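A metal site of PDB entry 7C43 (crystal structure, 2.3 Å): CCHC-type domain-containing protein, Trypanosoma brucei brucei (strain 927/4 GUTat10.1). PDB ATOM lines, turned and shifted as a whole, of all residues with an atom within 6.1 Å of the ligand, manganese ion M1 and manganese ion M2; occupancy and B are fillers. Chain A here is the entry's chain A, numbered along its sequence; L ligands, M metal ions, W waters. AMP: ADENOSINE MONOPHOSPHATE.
N of Ala 44 sits at hydrogen-bond distance from O3' of the ligand (2.8 Å).
N6 of the ligand is in hydrogen-bond range of OG1 of Thr 168 (3.4 Å).
O2' of the ligand lies within hydrogen-bond range of O of Ala 44 (2.7 Å).
O of Gln 164 lies within hydrogen-bond range of OG1 of Thr 168, at 2.8 Å.
O of Asp 41 lies within hydrogen-bond range of N of Gln 61, at 3.0 Å.
The backbone NH of Glu 43 lies close to the side-chain amide nitrogen of Gln 61.
The side-chain sulfur of Met 167 sits close to the indole nitrogen of Trp 175, at 3.7 Å.
The side-chain amide oxygen (OE1) of Gln 61 sits close to the backbone carbonyl oxygen (O) of Ala 188, 3.1 Å away.
The backbone carbonyl oxygen (O) of Met 167 sits close to a nitrogen (N1) of the ligand (3.3 Å).
Ile 42 touches the ligand (O to C5', 3.5 Å).
O of Phe 45 touches O2' of the ligand, 3.8 Å away.
Leu 54 touches the ligand (CD2 to O4', 3.7 Å).
NE1 of Trp 175 touches O3' of the ligand, 3.9 Å away.
Hydrophobic or aromatic side chains that line the ligand: Ala 44, Leu 54 and Met 167.
Within 4 Å of the ligand: Asp 41, Ile 42, Glu 43, Ala 44, Phe 45, Leu 54, Met 167, Thr 168, Trp 175 and Asp 191.
Gln 61 touches manganese ion M1.
Four residues have an atom within 4 Å of manganese ion M1: Asp 41, Glu 43, Gln 61 and Asp 191.
Asp 106 touches manganese ion M2.
Two residues have an atom within 4 Å of manganese ion M2: Asp 41 and Asp 106.
The nearest printed residue that does not touch manganese ion M2 is Asp 191 (4.2 Å).
O1P of the ligand binds manganese ion M1, 2.2 Å away.
The side-chain carboxylate (OD2) of Asp 41 binds manganese ion M1 (2.3 Å).
OD2 of Asp 191 is bound to manganese ion M1, 2.4 Å away.
The side-chain carboxylate (OE1) of Glu 43 is bound to manganese ion M1, at 2.7 Å.
Manganese ion M1 has four donor atoms within binding distance.
O1P of the ligand binds manganese ion M2, 2.1 Å away.
Water W3 is bound to manganese ion M2, 2.1 Å away.
OD1 of Asp 41 is bound to manganese ion M2 (2.1 Å).
Water W2 binds manganese ion M2, 2.2 Å away.
Slightly farther from manganese ion M2 lies an oxygen (O3P) of the ligand (2.8 Å).
Water W2 bridges the side-chain carboxylate (OD1) of Asp 106 and the backbone carbonyl oxygen (O) of Ile 42.
Water W1 lies within hydrogen-bond range of O2' of the ligand, O of Phe 45 and N of Gly 55.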
ATOM      1  N   LEU A  40      -1.237  26.577  16.485  1.00  0.00           N
ATOM      2  CA  LEU A  40      -1.455  27.325  17.712  1.00  0.00           C
ATOM      3  C   LEU A  40      -2.871  27.265  18.225  1.00  0.00           C
ATOM      4  O   LEU A  40      -3.803  27.016  17.481  1.00  0.00           O
ATOM      5  CB  LEU A  40      -1.092  28.781  17.524  1.00  0.00           C
ATOM      6  CG  LEU A  40       0.367  29.023  17.170  1.00  0.00           C
ATOM      7  CD1 LEU A  40       0.550  30.480  16.791  1.00  0.00           C
ATOM      8  CD2 LEU A  40       1.275  28.622  18.333  1.00  0.00           C
ATOM      9  N   ASP A  41      -3.001  27.464  19.530  1.00  0.00           N
ATOM     10  CA  ASP A  41      -4.284  27.600  20.148  1.00  0.00           C
ATOM     11  C   ASP A  41      -4.083  28.340  21.458  1.00  0.00           C
ATOM     12  O   ASP A  41      -2.956  28.406  21.942  1.00  0.00           O
ATOM     13  CB  ASP A  41      -4.897  26.223  20.401  1.00  0.00           C
ATOM     14  CG  ASP A  41      -6.389  26.285  20.709  1.00  0.00           C
ATOM     15  OD1 ASP A  41      -7.055  27.270  20.320  1.00  0.00           O
ATOM     16  OD2 ASP A  41      -6.882  25.316  21.313  1.00  0.00           O
ATOM     17  N   ILE A  42      -5.183  28.880  22.010  1.00  0.00           N
ATOM     18  CA  ILE A  42      -5.196  29.528  23.336  1.00  0.00           C
ATOM     19  C   ILE A  42      -6.242  28.909  24.267  1.00  0.00           C
ATOM     20  O   ILE A  42      -7.362  28.705  23.854  1.00  0.00           O
ATOM     21  CB  ILE A  42      -5.494  31.027  23.179  1.00  0.00           C
ATOM     22  CG1 ILE A  42      -4.408  31.684  22.309  1.00  0.00           C
ATOM     23  CG2 ILE A  42      -5.607  31.705  24.532  1.00  0.00           C
ATOM     24  CD1 ILE A  42      -4.566  33.190  22.103  1.00  0.00           C
ATOM     25  N   GLU A  43      -5.865  28.631  25.509  1.00  0.00           N
ATOM     26  CA  GLU A  43      -6.816  28.349  26.563  1.00  0.00           C
ATOM     27  C   GLU A  43      -6.829  29.584  27.416  1.00  0.00           C
ATOM     28  O   GLU A  43      -5.791  29.979  27.932  1.00  0.00           O
ATOM     29  CB  GLU A  43      -6.402  27.199  27.505  1.00  0.00           C
ATOM     30  CG  GLU A  43      -6.651  25.755  27.126  1.00  0.00           C
ATOM     31  CD  GLU A  43      -7.885  25.474  26.302  1.00  0.00           C
ATOM     32  OE1 GLU A  43      -7.759  24.723  25.309  1.00  0.00           O
ATOM     33  OE2 GLU A  43      -8.970  25.985  26.614  1.00  0.00           O
ATOM     34  N   ALA A  44      -8.034  30.122  27.662  1.00  0.00           N
ATOM     35  CA  ALA A  44      -8.235  31.331  28.433  1.00  0.00           C
ATOM     36  C   ALA A  44      -9.175  31.088  29.616  1.00  0.00           C
ATOM     37  O   ALA A  44      -9.931  30.112  29.622  1.00  0.00           O
ATOM     38  CB  ALA A  44      -8.813  32.386  27.522  1.00  0.00           C
ATOM     39  N   PHE A  45      -9.125  32.005  30.582  1.00  0.00           N
ATOM     40  CA  PHE A  45     -10.052  32.020  31.702  1.00  0.00           C
ATOM     41  C   PHE A  45     -11.461  32.165  31.154  1.00  0.00           C
ATOM     42  O   PHE A  45     -11.707  33.018  30.325  1.00  0.00           O
ATOM     43  CB  PHE A  45      -9.809  33.239  32.616  1.00  0.00           C
ATOM     44  CG  PHE A  45      -8.631  33.144  33.527  1.00  0.00           C
ATOM     45  CD1 PHE A  45      -7.594  32.212  33.330  1.00  0.00           C
ATOM     46  CD2 PHE A  45      -8.522  34.046  34.573  1.00  0.00           C
ATOM     47  CE1 PHE A  45      -6.503  32.166  34.186  1.00  0.00           C
ATOM     48  CE2 PHE A  45      -7.443  33.998  35.442  1.00  0.00           C
ATOM     49  CZ  PHE A  45      -6.416  33.068  35.243  1.00  0.00           C
ATOM     50  N   CYS A  46     -12.383  31.365  31.658  1.00  0.00           N
ATOM     51  CA  CYS A  46     -13.760  31.420  31.212  1.00  0.00           C
ATOM     52  C   CYS A  46     -14.394  32.708  31.634  1.00  0.00           C
ATOM     53  O   CYS A  46     -14.186  33.162  32.731  1.00  0.00           O
ATOM     54  CB  CYS A  46     -14.540  30.251  31.779  1.00  0.00           C
ATOM     55  SG  CYS A  46     -14.046  28.722  30.998  1.00  0.00           S
ATOM     56  N   THR A  47     -15.186  33.292  30.783  1.00  0.00           N
ATOM     57  CA  THR A  47     -15.835  34.509  31.142  1.00  0.00           C
ATOM     58  C   THR A  47     -17.232  34.188  31.627  1.00  0.00           C
ATOM     59  O   THR A  47     -17.986  33.507  30.974  1.00  0.00           O
ATOM     60  CB  THR A  47     -15.958  35.446  29.950  1.00  0.00           C
ATOM     61  OG1 THR A  47     -16.862  34.868  29.008  1.00  0.00           O
ATOM     62  CG2 THR A  47     -14.667  35.605  29.269  1.00  0.00           C
ATOM     63  N   LEU A  54     -12.058  36.449  24.555  1.00  0.00           N
ATOM     64  CA  LEU A  54     -11.450  35.517  25.485  1.00  0.00           C
ATOM     65  C   LEU A  54     -11.082  36.256  26.764  1.00  0.00           C
ATOM     66  O   LEU A  54     -10.673  37.391  26.736  1.00  0.00           O
ATOM     67  CB  LEU A  54     -10.165  34.905  24.910  1.00  0.00           C
ATOM     68  CG  LEU A  54     -10.215  33.980  23.693  1.00  0.00           C
ATOM     69  CD1 LEU A  54      -8.845  33.368  23.412  1.00  0.00           C
ATOM     70  CD2 LEU A  54     -11.244  32.881  23.897  1.00  0.00           C
ATOM     71  N   GLY A  55     -11.221  35.587  27.894  1.00  0.00           N
ATOM     72  CA  GLY A  55     -10.650  36.067  29.146  1.00  0.00           C
ATOM     73  C   GLY A  55      -9.136  35.955  29.161  1.00  0.00           C
ATOM     74  O   GLY A  55      -8.490  35.808  28.139  1.00  0.00           O
ATOM     75  N   GLN A  61      -0.818  26.908  23.328  1.00  0.00           N
ATOM     76  CA  GLN A  61      -0.448  25.565  22.981  1.00  0.00           C
ATOM     77  C   GLN A  61       0.165  25.613  21.595  1.00  0.00           C
ATOM     78  O   GLN A  61      -0.374  26.271  20.716  1.00  0.00           O
ATOM     79  CB  GLN A  61      -1.697  24.692  22.892  1.00  0.00           C
ATOM     80  CG  GLN A  61      -2.478  24.560  24.187  1.00  0.00           C
ATOM     81  CD  GLN A  61      -3.714  25.429  24.255  1.00  0.00           C
ATOM     82  OE1 GLN A  61      -4.816  25.001  23.955  1.00  0.00           O
ATOM     83  NE2 GLN A  61      -3.529  26.664  24.677  1.00  0.00           N
ATOM     84  N   PHE A 101      -7.428  26.967  14.117  1.00  0.00           N
ATOM     85  CA  PHE A 101      -8.840  26.643  13.819  1.00  0.00           C
ATOM     86  C   PHE A 101      -9.811  27.670  14.439  1.00  0.00           C
ATOM     87  O   PHE A 101     -10.089  27.652  15.639  1.00  0.00           O
ATOM     88  CB  PHE A 101      -9.160  25.216  14.271  1.00  0.00           C
ATOM     89  CG  PHE A 101     -10.440  24.674  13.687  1.00  0.00           C
ATOM     90  CD1 PHE A 101     -11.658  24.851  14.340  1.00  0.00           C
ATOM     91  CD2 PHE A 101     -10.423  23.965  12.479  1.00  0.00           C
ATOM     92  CE1 PHE A 101     -12.840  24.326  13.806  1.00  0.00           C
ATOM     93  CE2 PHE A 101     -11.602  23.448  11.940  1.00  0.00           C
ATOM     94  CZ  PHE A 101     -12.819  23.633  12.588  1.00  0.00           C
ATOM     95  N   ASP A 102     -10.348  28.535  13.587  1.00  0.00           N
ATOM     96  CA  ASP A 102     -11.061  29.772  13.991  1.00  0.00           C
ATOM     97  C   ASP A 102     -10.135  30.689  14.750  1.00  0.00           C
ATOM     98  O   ASP A 102     -10.059  30.601  15.964  1.00  0.00           O
ATOM     99  CB  ASP A 102     -12.336  29.516  14.814  1.00  0.00           C
ATOM    100  CG  ASP A 102     -13.162  30.773  15.005  1.00  0.00           C
ATOM    101  OD1 ASP A 102     -12.757  31.864  14.547  1.00  0.00           O
ATOM    102  OD2 ASP A 102     -14.235  30.696  15.616  1.00  0.00           O
ATOM    103  N   ASP A 106      -8.724  34.315  19.092  1.00  0.00           N
ATOM    104  CA  ASP A 106      -7.335  34.036  19.452  1.00  0.00           C
ATOM    105  C   ASP A 106      -6.462  35.204  19.039  1.00  0.00           C
ATOM    106  O   ASP A 106      -5.607  35.654  19.788  1.00  0.00           O
ATOM    107  CB  ASP A 106      -6.830  32.754  18.767  1.00  0.00           C
ATOM    108  CG  ASP A 106      -7.439  31.473  19.359  1.00  0.00           C
ATOM    109  OD1 ASP A 106      -7.986  31.504  20.488  1.00  0.00           O
ATOM    110  OD2 ASP A 106      -7.349  30.406  18.699  1.00  0.00           O
ATOM    111  N   GLN A 164     -14.921  20.165  30.077  1.00  0.00           N
ATOM    112  CA  GLN A 164     -15.949  20.767  29.258  1.00  0.00           C
ATOM    113  C   GLN A 164     -17.146  21.244  30.080  1.00  0.00           C
ATOM    114  O   GLN A 164     -17.708  22.288  29.751  1.00  0.00           O
ATOM    115  CB  GLN A 164     -16.400  19.772  28.192  1.00  0.00           C
ATOM    116  CG  GLN A 164     -17.481  20.291  27.271  1.00  0.00           C
ATOM    117  CD  GLN A 164     -17.839  19.297  26.206  1.00  0.00           C
ATOM    118  OE1 GLN A 164     -17.416  18.127  26.247  1.00  0.00           O
ATOM    119  NE2 GLN A 164     -18.619  19.742  25.230  1.00  0.00           N
ATOM    120  N   MET A 167     -16.261  24.433  32.149  1.00  0.00           N
ATOM    121  CA  MET A 167     -16.212  25.538  31.209  1.00  0.00           C
ATOM    122  C   MET A 167     -17.600  25.988  30.838  1.00  0.00           C
ATOM    123  O   MET A 167     -17.889  27.178  30.905  1.00  0.00           O
ATOM    124  CB  MET A 167     -15.438  25.180  29.931  1.00  0.00           C
ATOM    125  CG  MET A 167     -13.922  25.149  30.119  1.00  0.00           C
ATOM    126  SD  MET A 167     -13.037  25.117  28.341  1.00  0.00           S
ATOM    127  CE  MET A 167     -11.964  23.557  28.760  1.00  0.00           C
ATOM    128  N   THR A 168     -18.473  25.051  30.443  1.00  0.00           N
ATOM    129  CA  THR A 168     -19.830  25.429  29.965  1.00  0.00           C
ATOM    130  C   THR A 168     -20.678  26.102  31.061  1.00  0.00           C
ATOM    131  O   THR A 168     -21.512  26.951  30.751  1.00  0.00           O
ATOM    132  CB  THR A 168     -20.614  24.234  29.319  1.00  0.00           C
ATOM    133  OG1 THR A 168     -19.777  23.551  28.381  1.00  0.00           O
ATOM    134  CG2 THR A 168     -21.884  24.741  28.577  1.00  0.00           C
ATOM    135  N   LEU A 169     -20.462  25.751  32.333  1.00  0.00           N
ATOM    136  CA  LEU A 169     -21.157  26.423  33.432  1.00  0.00           C
ATOM    137  C   LEU A 169     -20.864  27.946  33.483  1.00  0.00           C
ATOM    138  O   LEU A 169     -21.775  28.747  33.716  1.00  0.00           O
ATOM    139  CB  LEU A 169     -20.885  25.743  34.776  1.00  0.00           C
ATOM    140  CG  LEU A 169     -21.919  26.019  35.888  1.00  0.00           C
ATOM    141  CD1 LEU A 169     -23.358  25.732  35.461  1.00  0.00           C
ATOM    142  CD2 LEU A 169     -21.562  25.220  37.130  1.00  0.00           C
ATOM    143  N   GLY A 170     -19.609  28.334  33.247  1.00  0.00           N
ATOM    144  CA  GLY A 170     -19.244  29.743  32.982  1.00  0.00           C
ATOM    145  C   GLY A 170     -19.209  30.683  34.179  1.00  0.00           C
ATOM    146  O   GLY A 170     -19.114  31.913  34.018  1.00  0.00           O
ATOM    147  N   TRP A 175      -9.285  27.792  34.207  1.00  0.00           N
ATOM    148  CA  TRP A 175      -7.934  27.710  33.768  1.00  0.00           C
ATOM    149  C   TRP A 175      -6.941  28.433  34.611  1.00  0.00           C
ATOM    150  O   TRP A 175      -5.801  28.498  34.266  1.00  0.00           O
ATOM    151  CB  TRP A 175      -7.855  28.118  32.338  1.00  0.00           C
ATOM    152  CG  TRP A 175      -8.478  27.135  31.438  1.00  0.00           C
ATOM    153  CD1 TRP A 175      -9.660  27.242  30.823  1.00  0.00           C
ATOM    154  CD2 TRP A 175      -7.970  25.865  31.073  1.00  0.00           C
ATOM    155  NE1 TRP A 175      -9.924  26.155  30.099  1.00  0.00           N
ATOM    156  CE2 TRP A 175      -8.898  25.280  30.229  1.00  0.00           C
ATOM    157  CE3 TRP A 175      -6.812  25.170  31.378  1.00  0.00           C
ATOM    158  CZ2 TRP A 175      -8.710  24.049  29.694  1.00  0.00           C
ATOM    159  CZ3 TRP A 175      -6.630  23.963  30.840  1.00  0.00           C
ATOM    160  CH2 TRP A 175      -7.564  23.411  30.010  1.00  0.00           C
ATOM    161  N   TYR A 187      -6.430  17.882  27.800  1.00  0.00           N
ATOM    162  CA  TYR A 187      -7.505  18.609  27.127  1.00  0.00           C
ATOM    163  C   TYR A 187      -6.935  19.729  26.292  1.00  0.00           C
ATOM    164  O   TYR A 187      -7.313  19.890  25.133  1.00  0.00           O
ATOM    165  CB  TYR A 187      -8.531  19.194  28.121  1.00  0.00           C
ATOM    166  CG  TYR A 187      -9.801  19.728  27.502  1.00  0.00           C
ATOM    167  CD1 TYR A 187      -9.823  20.924  26.762  1.00  0.00           C
ATOM    168  CD2 TYR A 187     -11.007  19.042  27.662  1.00  0.00           C
ATOM    169  CE1 TYR A 187     -11.016  21.411  26.197  1.00  0.00           C
ATOM    170  CE2 TYR A 187     -12.195  19.521  27.126  1.00  0.00           C
ATOM    171  CZ  TYR A 187     -12.189  20.699  26.386  1.00  0.00           C
ATOM    172  OH  TYR A 187     -13.386  21.139  25.861  1.00  0.00           O
ATOM    173  N   ALA A 188      -6.024  20.500  26.882  1.00  0.00           N
ATOM    174  CA  ALA A 188      -5.391  21.629  26.207  1.00  0.00           C
ATOM    175  C   ALA A 188      -4.591  21.230  24.990  1.00  0.00           C
ATOM    176  O   ALA A 188      -4.594  21.939  23.985  1.00  0.00           O
ATOM    177  CB  ALA A 188      -4.498  22.384  27.158  1.00  0.00           C
ATOM    178  N   ASP A 191      -6.511  20.176  20.736  1.00  0.00           N
ATOM    179  CA  ASP A 191      -6.791  20.958  19.517  1.00  0.00           C
ATOM    180  C   ASP A 191      -5.596  21.133  18.567  1.00  0.00           C
ATOM    181  O   ASP A 191      -5.769  21.015  17.348  1.00  0.00           O
ATOM    182  CB  ASP A 191      -7.358  22.337  19.862  1.00  0.00           C
ATOM    183  CG  ASP A 191      -8.819  22.302  20.358  1.00  0.00           C
ATOM    184  OD1 ASP A 191      -9.479  21.247  20.215  1.00  0.00           O
ATOM    185  OD2 ASP A 191      -9.292  23.357  20.878  1.00  0.00           O
HETATM  186  P   AMP L   1     -11.117  26.335  22.075  1.00  0.00           P
HETATM  187  O1P AMP L   1      -9.646  26.308  21.816  1.00  0.00           O
HETATM  188  O2P AMP L   1     -11.496  24.900  22.251  1.00  0.00           O
HETATM  189  O3P AMP L   1     -11.771  27.128  20.995  1.00  0.00           O
HETATM  190  O5' AMP L   1     -11.350  27.111  23.460  1.00  0.00           O
HETATM  191  C5' AMP L   1     -10.858  28.460  23.644  1.00  0.00           C
HETATM  192  C4' AMP L   1     -11.313  29.123  24.929  1.00  0.00           C
HETATM  193  O4' AMP L   1     -12.681  29.579  24.813  1.00  0.00           O
HETATM  194  C3' AMP L   1     -11.282  28.326  26.235  1.00  0.00           C
HETATM  195  O3' AMP L   1      -9.999  28.258  26.839  1.00  0.00           O
HETATM  196  C2' AMP L   1     -12.262  29.125  27.088  1.00  0.00           C
HETATM  197  O2' AMP L   1     -11.789  30.339  27.634  1.00  0.00           O
HETATM  198  C1' AMP L   1     -13.343  29.449  26.062  1.00  0.00           C
HETATM  199  N9  AMP L   1     -14.318  28.368  25.941  1.00  0.00           N
HETATM  200  C8  AMP L   1     -14.206  27.230  25.172  1.00  0.00           C
HETATM  201  N7  AMP L   1     -15.236  26.418  25.295  1.00  0.00           N
HETATM  202  C5  AMP L   1     -16.064  27.064  26.197  1.00  0.00           C
HETATM  203  C6  AMP L   1     -17.320  26.716  26.736  1.00  0.00           C
HETATM  204  N6  AMP L   1     -17.968  25.601  26.419  1.00  0.00           N
HETATM  205  N1  AMP L   1     -17.882  27.576  27.607  1.00  0.00           N
HETATM  206  C2  AMP L   1     -17.222  28.697  27.921  1.00  0.00           C
HETATM  207  N3  AMP L   1     -16.035  29.134  27.479  1.00  0.00           N
HETATM  208  C4  AMP L   1     -15.506  28.257  26.605  1.00  0.00           C
HETATM  209 MN    MN M   1      -8.572  24.606  22.754  1.00  0.00          MN
HETATM  210 MN    MN M   2      -9.171  27.520  20.162  1.00  0.00          MN
HETATM  211  O   HOH W   1     -12.405  32.751  27.630  1.00  0.00           O
HETATM  212  O   HOH W   2      -8.645  29.199  21.422  1.00  0.00           O
HETATM  213  O   HOH W   3      -9.180  28.821  18.492  1.00  0.00           O
